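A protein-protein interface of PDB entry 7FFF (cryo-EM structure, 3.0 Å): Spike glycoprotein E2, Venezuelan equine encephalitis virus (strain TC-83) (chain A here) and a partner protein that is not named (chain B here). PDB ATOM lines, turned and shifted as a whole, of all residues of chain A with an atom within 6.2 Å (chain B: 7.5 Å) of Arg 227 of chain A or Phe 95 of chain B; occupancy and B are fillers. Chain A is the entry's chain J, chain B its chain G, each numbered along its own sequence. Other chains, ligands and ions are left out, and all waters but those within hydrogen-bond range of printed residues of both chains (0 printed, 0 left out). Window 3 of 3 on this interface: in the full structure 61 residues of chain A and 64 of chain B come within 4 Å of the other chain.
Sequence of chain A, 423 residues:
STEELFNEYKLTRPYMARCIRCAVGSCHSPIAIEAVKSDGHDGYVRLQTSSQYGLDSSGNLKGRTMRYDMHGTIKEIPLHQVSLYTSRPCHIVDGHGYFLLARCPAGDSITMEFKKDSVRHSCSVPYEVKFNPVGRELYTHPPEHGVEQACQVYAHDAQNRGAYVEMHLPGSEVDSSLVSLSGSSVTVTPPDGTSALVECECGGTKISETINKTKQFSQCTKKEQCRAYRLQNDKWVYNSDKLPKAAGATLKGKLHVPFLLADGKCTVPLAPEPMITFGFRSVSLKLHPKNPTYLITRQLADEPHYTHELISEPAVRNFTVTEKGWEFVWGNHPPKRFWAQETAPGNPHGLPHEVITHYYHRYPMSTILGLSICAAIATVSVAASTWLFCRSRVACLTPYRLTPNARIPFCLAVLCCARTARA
The backbone carbonyl oxygen (O) of Val 174 of chain A lies close to the backbone carbonyl oxygen (O) of Gly 90 of chain B (2.9 Å).
The backbone carbonyl oxygen of Cys 94 of chain B sits at hydrogen-bond distance from the guanidinium group of Arg 227 of chain A.
OH of Tyr 229 of chain A lies within hydrogen-bond range of O of Tyr 93 of chain B, at 3.1 Å.
SG of Cys 200 of chain A forms a disulfide with SG of Cys 226 of chain A (2.0 Å).
The backbone carbonyl oxygen (O) of Glu 201 of chain A sits close to the side-chain amide oxygen (OE1) of Gln 225 of chain A.
The side-chain sulfur of Cys 96 of chain B is disulfide-bonded to the side-chain sulfur of Cys 63 of chain B (2.0 Å).
OD1 of Asn 100 of chain B lies close to SG of Cys 94 of chain B, at 3.5 Å.
The backbone carbonyl oxygen (O) of Glu 224 of chain A lies within hydrogen-bond range of the guanidinium group (NH1) of Arg 227 of chain A.
The backbone NH (N) of Tyr 229 of chain A is in hydrogen-bond range of the backbone carbonyl oxygen (O) of Leu 197 of chain A (2.8 Å).
Among the printed residues, merely in contact across the chains: Val 174 of chain A with Ala 92 of chain B, Arg 227 of chain A with Phe 95 of chain B, Glu 201 of chain A with Phe 95 of chain B, Arg 227 of chain A with Tyr 85 of chain B, Val 174 of chain A with Tyr 93 of chain B, Arg 227 of chain A with Ala 92 of chain B, Arg 227 of chain A with Tyr 93 of chain B, Val 174 of chain A with Gly 91 of chain B and Tyr 229 of chain A with Cys 62 of chain B.
Of the printed residues of chain B, Val 174 of chain A touches Gly 90 (2.9 Å), Gly 91 (3.9 Å), Ala 92 (3.1 Å) and Tyr 93 (3.9 Å).
Of chain B, only Tyr 85 (3.6 Å), Ala 92 (3.9 Å), Tyr 93 (3.9 Å), Cys 94 (2.9 Å) and Phe 95 (3.4 Å) come within 4 Å of Arg 227 of chain A.
Of the printed residues of chain B, Tyr 229 of chain A touches Cys 62 and Tyr 93.
Of the printed residues of chain A, Cys 62 of chain B touches Tyr 229 (3.998 Å).
Printed residues of chain A within 4 Å of Tyr 85 of chain B: Arg 227.
Of the printed residues of chain A, Gly 90 of chain B touches Val 174.
Of chain A, only Glu 201 (3.5 Å) and Arg 227 (3.4 Å) come within 4 Å of Phe 95 of chain B.
The nearest printed residue of chain A that does not touch Cys 62 of chain B is Glu 199 of chain A (5.3 Å).
Of the 13 printed residues of chain A, 4 touch a printed residue of chain B.
Printed residues of chain A that touch a printed residue of chain B: Val 174, Glu 201, Arg 227 and Tyr 229.
Hydrophobic or aromatic side chains of chain B within 4 Å of the printed part of chain A: Tyr 85 and Phe 95.
Among the printed residues, 12 pairs touch across the chains.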
ATOM      1  N   VAL A 174       8.191  13.031   8.107  1.00  0.00           N
ATOM      2  CA  VAL A 174       6.777  13.319   8.216  1.00  0.00           C
ATOM      3  C   VAL A 174       6.343  13.052   9.642  1.00  0.00           C
ATOM      4  O   VAL A 174       6.654  12.001  10.198  1.00  0.00           O
ATOM      5  CB  VAL A 174       5.960  12.425   7.271  1.00  0.00           C
ATOM      6  CG1 VAL A 174       6.392  10.976   7.416  1.00  0.00           C
ATOM      7  CG2 VAL A 174       4.472  12.574   7.548  1.00  0.00           C
ATOM      8  N   LEU A 197       6.570  21.945   6.460  1.00  0.00           N
ATOM      9  CA  LEU A 197       5.887  22.128   5.189  1.00  0.00           C
ATOM     10  C   LEU A 197       4.794  21.085   5.082  1.00  0.00           C
ATOM     11  O   LEU A 197       4.922  19.976   5.602  1.00  0.00           O
ATOM     12  CB  LEU A 197       6.809  22.037   3.967  1.00  0.00           C
ATOM     13  CG  LEU A 197       7.395  20.720   3.491  1.00  0.00           C
ATOM     14  CD1 LEU A 197       7.711  20.847   2.025  1.00  0.00           C
ATOM     15  CD2 LEU A 197       8.665  20.470   4.251  1.00  0.00           C
ATOM     16  N   VAL A 198       3.716  21.460   4.405  1.00  0.00           N
ATOM     17  CA  VAL A 198       2.527  20.632   4.274  1.00  0.00           C
ATOM     18  C   VAL A 198       2.294  20.395   2.794  1.00  0.00           C
ATOM     19  O   VAL A 198       2.352  21.337   1.997  1.00  0.00           O
ATOM     20  CB  VAL A 198       1.306  21.304   4.924  1.00  0.00           C
ATOM     21  CG1 VAL A 198       0.075  20.436   4.804  1.00  0.00           C
ATOM     22  CG2 VAL A 198       1.589  21.612   6.363  1.00  0.00           C
ATOM     23  N   GLU A 199       2.047  19.144   2.419  1.00  0.00           N
ATOM     24  CA  GLU A 199       1.691  18.815   1.047  1.00  0.00           C
ATOM     25  C   GLU A 199       0.390  18.033   1.043  1.00  0.00           C
ATOM     26  O   GLU A 199       0.274  17.014   1.729  1.00  0.00           O
ATOM     27  CB  GLU A 199       2.785  18.007   0.350  1.00  0.00           C
ATOM     28  CG  GLU A 199       4.061  18.778   0.105  1.00  0.00           C
ATOM     29  CD  GLU A 199       5.065  17.978  -0.688  1.00  0.00           C
ATOM     30  OE1 GLU A 199       4.777  16.802  -0.990  1.00  0.00           O
ATOM     31  OE2 GLU A 199       6.144  18.520  -1.003  1.00  0.00           O
ATOM     32  N   CYS A 200      -0.580  18.510   0.271  1.00  0.00           N
ATOM     33  CA  CYS A 200      -1.898  17.905   0.205  1.00  0.00           C
ATOM     34  C   CYS A 200      -2.259  17.674  -1.253  1.00  0.00           C
ATOM     35  O   CYS A 200      -1.720  18.320  -2.155  1.00  0.00           O
ATOM     36  CB  CYS A 200      -2.956  18.802   0.858  1.00  0.00           C
ATOM     37  SG  CYS A 200      -2.582  19.301   2.542  1.00  0.00           S
ATOM     38  N   GLU A 201      -3.175  16.737  -1.484  1.00  0.00           N
ATOM     39  CA  GLU A 201      -3.871  16.642  -2.761  1.00  0.00           C
ATOM     40  C   GLU A 201      -5.358  16.463  -2.496  1.00  0.00           C
ATOM     41  O   GLU A 201      -6.021  15.555  -2.993  1.00  0.00           O
ATOM     42  CB  GLU A 201      -3.292  15.533  -3.639  1.00  0.00           C
ATOM     43  CG  GLU A 201      -3.489  15.734  -5.153  1.00  0.00           C
ATOM     44  CD  GLU A 201      -4.734  15.075  -5.719  1.00  0.00           C
ATOM     45  OE1 GLU A 201      -5.129  14.004  -5.218  1.00  0.00           O
ATOM     46  OE2 GLU A 201      -5.324  15.628  -6.669  1.00  0.00           O
ATOM     47  N   LYS A 223      -7.853  14.500   7.097  1.00  0.00           N
ATOM     48  CA  LYS A 223      -6.445  14.732   7.394  1.00  0.00           C
ATOM     49  C   LYS A 223      -5.531  13.701   6.755  1.00  0.00           C
ATOM     50  O   LYS A 223      -4.311  13.880   6.769  1.00  0.00           O
ATOM     51  CB  LYS A 223      -6.225  14.763   8.906  1.00  0.00           C
ATOM     52  CG  LYS A 223      -6.549  13.471   9.613  1.00  0.00           C
ATOM     53  CD  LYS A 223      -6.360  13.641  11.107  1.00  0.00           C
ATOM     54  CE  LYS A 223      -6.669  12.364  11.857  1.00  0.00           C
ATOM     55  NZ  LYS A 223      -6.484  12.550  13.323  1.00  0.00           N
ATOM     56  N   GLU A 224      -6.094  12.641   6.183  1.00  0.00           N
ATOM     57  CA  GLU A 224      -5.359  11.681   5.376  1.00  0.00           C
ATOM     58  C   GLU A 224      -5.063  12.198   3.977  1.00  0.00           C
ATOM     59  O   GLU A 224      -4.386  11.513   3.207  1.00  0.00           O
ATOM     60  CB  GLU A 224      -6.156  10.385   5.293  1.00  0.00           C
ATOM     61  CG  GLU A 224      -6.346   9.729   6.639  1.00  0.00           C
ATOM     62  CD  GLU A 224      -7.251   8.528   6.565  1.00  0.00           C
ATOM     63  OE1 GLU A 224      -7.831   8.296   5.484  1.00  0.00           O
ATOM     64  OE2 GLU A 224      -7.388   7.821   7.583  1.00  0.00           O
ATOM     65  N   GLN A 225      -5.571  13.378   3.625  1.00  0.00           N
ATOM     66  CA  GLN A 225      -5.206  14.034   2.381  1.00  0.00           C
ATOM     67  C   GLN A 225      -3.873  14.759   2.477  1.00  0.00           C
ATOM     68  O   GLN A 225      -3.261  15.038   1.445  1.00  0.00           O
ATOM     69  CB  GLN A 225      -6.286  15.042   1.978  1.00  0.00           C
ATOM     70  CG  GLN A 225      -7.654  14.456   1.653  1.00  0.00           C
ATOM     71  CD  GLN A 225      -7.667  13.669   0.360  1.00  0.00           C
ATOM     72  OE1 GLN A 225      -7.006  14.036  -0.609  1.00  0.00           O
ATOM     73  NE2 GLN A 225      -8.438  12.591   0.331  1.00  0.00           N
ATOM     74  N   CYS A 226      -3.418  15.071   3.687  1.00  0.00           N
ATOM     75  CA  CYS A 226      -2.307  15.992   3.889  1.00  0.00           C
ATOM     76  C   CYS A 226      -1.154  15.321   4.615  1.00  0.00           C
ATOM     77  O   CYS A 226      -1.358  14.568   5.572  1.00  0.00           O
ATOM     78  CB  CYS A 226      -2.764  17.220   4.670  1.00  0.00           C
ATOM     79  SG  CYS A 226      -3.861  18.269   3.726  1.00  0.00           S
ATOM     80  N   ARG A 227       0.057  15.626   4.160  1.00  0.00           N
ATOM     81  CA  ARG A 227       1.292  15.126   4.744  1.00  0.00           C
ATOM     82  C   ARG A 227       2.102  16.319   5.230  1.00  0.00           C
ATOM     83  O   ARG A 227       2.479  17.181   4.430  1.00  0.00           O
ATOM     84  CB  ARG A 227       2.090  14.320   3.721  1.00  0.00           C
ATOM     85  CG  ARG A 227       1.397  13.077   3.206  1.00  0.00           C
ATOM     86  CD  ARG A 227       1.402  11.965   4.223  1.00  0.00           C
ATOM     87  NE  ARG A 227       0.864  10.735   3.659  1.00  0.00           N
ATOM     88  CZ  ARG A 227      -0.391  10.337   3.804  1.00  0.00           C
ATOM     89  NH1 ARG A 227      -1.236  11.060   4.514  1.00  0.00           N
ATOM     90  NH2 ARG A 227      -0.797   9.206   3.255  1.00  0.00           N
ATOM     91  N   ALA A 228       2.369  16.370   6.527  1.00  0.00           N
ATOM     92  CA  ALA A 228       3.169  17.430   7.124  1.00  0.00           C
ATOM     93  C   ALA A 228       4.552  16.885   7.439  1.00  0.00           C
ATOM     94  O   ALA A 228       4.675  15.795   8.006  1.00  0.00           O
ATOM     95  CB  ALA A 228       2.508  17.971   8.389  1.00  0.00           C
ATOM     96  N   TYR A 229       5.585  17.639   7.082  1.00  0.00           N
ATOM     97  CA  TYR A 229       6.961  17.232   7.307  1.00  0.00           C
ATOM     98  C   TYR A 229       7.576  18.069   8.421  1.00  0.00           C
ATOM     99  O   TYR A 229       6.922  18.918   9.024  1.00  0.00           O
ATOM    100  CB  TYR A 229       7.769  17.358   6.022  1.00  0.00           C
ATOM    101  CG  TYR A 229       7.288  16.459   4.918  1.00  0.00           C
ATOM    102  CD1 TYR A 229       7.603  15.112   4.907  1.00  0.00           C
ATOM    103  CD2 TYR A 229       6.526  16.957   3.876  1.00  0.00           C
ATOM    104  CE1 TYR A 229       7.164  14.284   3.894  1.00  0.00           C
ATOM    105  CE2 TYR A 229       6.088  16.141   2.859  1.00  0.00           C
ATOM    106  CZ  TYR A 229       6.411  14.804   2.874  1.00  0.00           C
ATOM    107  OH  TYR A 229       5.972  13.985   1.861  1.00  0.00           O
ATOM    108  N   CYS B  62       7.791  11.505  -4.176  1.00  0.00           N
ATOM    109  CA  CYS B  62       6.378  11.186  -4.005  1.00  0.00           C
ATOM    110  C   CYS B  62       5.629  11.496  -5.295  1.00  0.00           C
ATOM    111  O   CYS B  62       5.494  12.663  -5.669  1.00  0.00           O
ATOM    112  CB  CYS B  62       5.789  11.960  -2.829  1.00  0.00           C
ATOM    113  SG  CYS B  62       6.403  11.461  -1.209  1.00  0.00           S
ATOM    114  N   CYS B  63       5.124  10.443  -5.947  1.00  0.00           N
ATOM    115  CA  CYS B  63       4.431  10.502  -7.238  1.00  0.00           C
ATOM    116  C   CYS B  63       5.244  11.253  -8.296  1.00  0.00           C
ATOM    117  O   CYS B  63       4.885  12.330  -8.761  1.00  0.00           O
ATOM    118  CB  CYS B  63       3.022  11.084  -7.092  1.00  0.00           C
ATOM    119  SG  CYS B  63       1.753   9.820  -6.818  1.00  0.00           S
ATOM    120  N   TYR B  85       5.697   2.231  -1.061  1.00  0.00           N
ATOM    121  CA  TYR B  85       4.898   2.977  -0.092  1.00  0.00           C
ATOM    122  C   TYR B  85       5.669   3.033   1.213  1.00  0.00           C
ATOM    123  O   TYR B  85       5.407   2.258   2.137  1.00  0.00           O
ATOM    124  CB  TYR B  85       3.518   2.346   0.094  1.00  0.00           C
ATOM    125  CG  TYR B  85       2.576   3.232   0.867  1.00  0.00           C
ATOM    126  CD1 TYR B  85       1.996   4.336   0.266  1.00  0.00           C
ATOM    127  CD2 TYR B  85       2.273   2.978   2.198  1.00  0.00           C
ATOM    128  CE1 TYR B  85       1.147   5.154   0.959  1.00  0.00           C
ATOM    129  CE2 TYR B  85       1.419   3.799   2.895  1.00  0.00           C
ATOM    130  CZ  TYR B  85       0.865   4.890   2.264  1.00  0.00           C
ATOM    131  OH  TYR B  85       0.010   5.718   2.946  1.00  0.00           O
ATOM    132  N   PRO B  86       6.620   3.953   1.333  1.00  0.00           N
ATOM    133  CA  PRO B  86       7.539   3.934   2.472  1.00  0.00           C
ATOM    134  C   PRO B  86       6.909   4.500   3.734  1.00  0.00           C
ATOM    135  O   PRO B  86       5.822   5.074   3.715  1.00  0.00           O
ATOM    136  CB  PRO B  86       8.695   4.816   1.994  1.00  0.00           C
ATOM    137  CG  PRO B  86       8.057   5.765   1.086  1.00  0.00           C
ATOM    138  CD  PRO B  86       6.956   5.028   0.386  1.00  0.00           C
ATOM    139  N   GLY B  90       6.811   8.802  11.956  1.00  0.00           N
ATOM    140  CA  GLY B  90       5.630   9.636  11.938  1.00  0.00           C
ATOM    141  C   GLY B  90       4.705   9.317  10.784  1.00  0.00           C
ATOM    142  O   GLY B  90       4.426  10.184   9.955  1.00  0.00           O
ATOM    143  N   GLY B  91       4.251   8.078  10.694  1.00  0.00           N
ATOM    144  CA  GLY B  91       3.275   7.712   9.693  1.00  0.00           C
ATOM    145  C   GLY B  91       3.879   7.493   8.326  1.00  0.00           C
ATOM    146  O   GLY B  91       5.087   7.343   8.151  1.00  0.00           O
ATOM    147  N   ALA B  92       2.993   7.474   7.335  1.00  0.00           N
ATOM    148  CA  ALA B  92       3.396   7.298   5.950  1.00  0.00           C
ATOM    149  C   ALA B  92       4.181   8.500   5.453  1.00  0.00           C
ATOM    150  O   ALA B  92       4.002   9.624   5.922  1.00  0.00           O
ATOM    151  CB  ALA B  92       2.180   7.083   5.059  1.00  0.00           C
ATOM    152  N   TYR B  93       5.063   8.255   4.485  1.00  0.00           N
ATOM    153  CA  TYR B  93       5.907   9.311   3.942  1.00  0.00           C
ATOM    154  C   TYR B  93       5.226   9.989   2.759  1.00  0.00           C
ATOM    155  O   TYR B  93       4.951  11.191   2.798  1.00  0.00           O
ATOM    156  CB  TYR B  93       7.253   8.730   3.508  1.00  0.00           C
ATOM    157  CG  TYR B  93       8.311   9.738   3.129  1.00  0.00           C
ATOM    158  CD1 TYR B  93       9.149  10.284   4.088  1.00  0.00           C
ATOM    159  CD2 TYR B  93       8.471  10.143   1.811  1.00  0.00           C
ATOM    160  CE1 TYR B  93      10.124  11.190   3.741  1.00  0.00           C
ATOM    161  CE2 TYR B  93       9.434  11.055   1.458  1.00  0.00           C
ATOM    162  CZ  TYR B  93      10.260  11.573   2.423  1.00  0.00           C
ATOM    163  OH  TYR B  93      11.225  12.482   2.067  1.00  0.00           O
ATOM    164  N   CYS B  94       4.959   9.232   1.705  1.00  0.00           N
ATOM    165  CA  CYS B  94       4.187   9.745   0.589  1.00  0.00           C
ATOM    166  C   CYS B  94       2.707   9.536   0.866  1.00  0.00           C
ATOM    167  O   CYS B  94       2.315   8.977   1.889  1.00  0.00           O
ATOM    168  CB  CYS B  94       4.605   9.063  -0.709  1.00  0.00           C
ATOM    169  SG  CYS B  94       6.288   9.434  -1.240  1.00  0.00           S
ATOM    170  N   PHE B  95       1.870  10.005  -0.056  1.00  0.00           N
ATOM    171  CA  PHE B  95       0.429   9.869   0.100  1.00  0.00           C
ATOM    172  C   PHE B  95      -0.253   9.200  -1.084  1.00  0.00           C
ATOM    173  O   PHE B  95      -1.480   9.072  -1.074  1.00  0.00           O
ATOM    174  CB  PHE B  95      -0.220  11.234   0.378  1.00  0.00           C
ATOM    175  CG  PHE B  95       0.021  12.268  -0.684  1.00  0.00           C
ATOM    176  CD1 PHE B  95       1.121  13.108  -0.612  1.00  0.00           C
ATOM    177  CD2 PHE B  95      -0.868  12.431  -1.730  1.00  0.00           C
ATOM    178  CE1 PHE B  95       1.343  14.064  -1.577  1.00  0.00           C
ATOM    179  CE2 PHE B  95      -0.644  13.376  -2.697  1.00  0.00           C
ATOM    180  CZ  PHE B  95       0.457  14.198  -2.619  1.00  0.00           C
ATOM    181  N   CYS B  96       0.495   8.768  -2.089  1.00  0.00           N
ATOM    182  CA  CYS B  96      -0.048   8.045  -3.226  1.00  0.00           C
ATOM    183  C   CYS B  96      -0.114   6.551  -2.916  1.00  0.00           C
ATOM    184  O   CYS B  96       0.426   6.082  -1.916  1.00  0.00           O
ATOM    185  CB  CYS B  96       0.823   8.272  -4.453  1.00  0.00           C
ATOM    186  SG  CYS B  96       1.088  10.002  -4.912  1.00  0.00           S
ATOM    187  N   ASP B  97      -0.772   5.796  -3.791  1.00  0.00           N
ATOM    188  CA  ASP B  97      -0.809   4.346  -3.615  1.00  0.00           C
ATOM    189  C   ASP B  97       0.227   3.640  -4.480  1.00  0.00           C
ATOM    190  O   ASP B  97       0.904   2.719  -4.019  1.00  0.00           O
ATOM    191  CB  ASP B  97      -2.206   3.808  -3.928  1.00  0.00           C
ATOM    192  CG  ASP B  97      -3.210   4.147  -2.855  1.00  0.00           C
ATOM    193  OD1 ASP B  97      -2.809   4.248  -1.679  1.00  0.00           O
ATOM    194  OD2 ASP B  97      -4.400   4.317  -3.191  1.00  0.00           O
ATOM    195  N   THR B  98       0.342   4.044  -5.735  1.00  0.00           N
ATOM    196  CA  THR B  98       1.388   3.575  -6.626  1.00  0.00           C
ATOM    197  C   THR B  98       2.249   4.767  -7.027  1.00  0.00           C
ATOM    198  O   THR B  98       2.135   5.855  -6.457  1.00  0.00           O
ATOM    199  CB  THR B  98       0.800   2.880  -7.857  1.00  0.00           C
ATOM    200  OG1 THR B  98      -0.016   3.805  -8.584  1.00  0.00           O
ATOM    201  CG2 THR B  98      -0.033   1.682  -7.448  1.00  0.00           C
ATOM    202  N   ASN B 100       5.209   5.772  -6.606  1.00  0.00           N
ATOM    203  CA  ASN B 100       6.319   6.303  -5.836  1.00  0.00           C
ATOM    204  C   ASN B 100       7.582   5.555  -6.223  1.00  0.00           C
ATOM    205  O   ASN B 100       7.537   4.418  -6.697  1.00  0.00           O
ATOM    206  CB  ASN B 100       6.072   6.181  -4.336  1.00  0.00           C
ATOM    207  CG  ASN B 100       4.972   7.087  -3.849  1.00  0.00           C
ATOM    208  OD1 ASN B 100       4.876   8.237  -4.258  1.00  0.00           O
ATOM    209  ND2 ASN B 100       4.135   6.571  -2.964  1.00  0.00           N
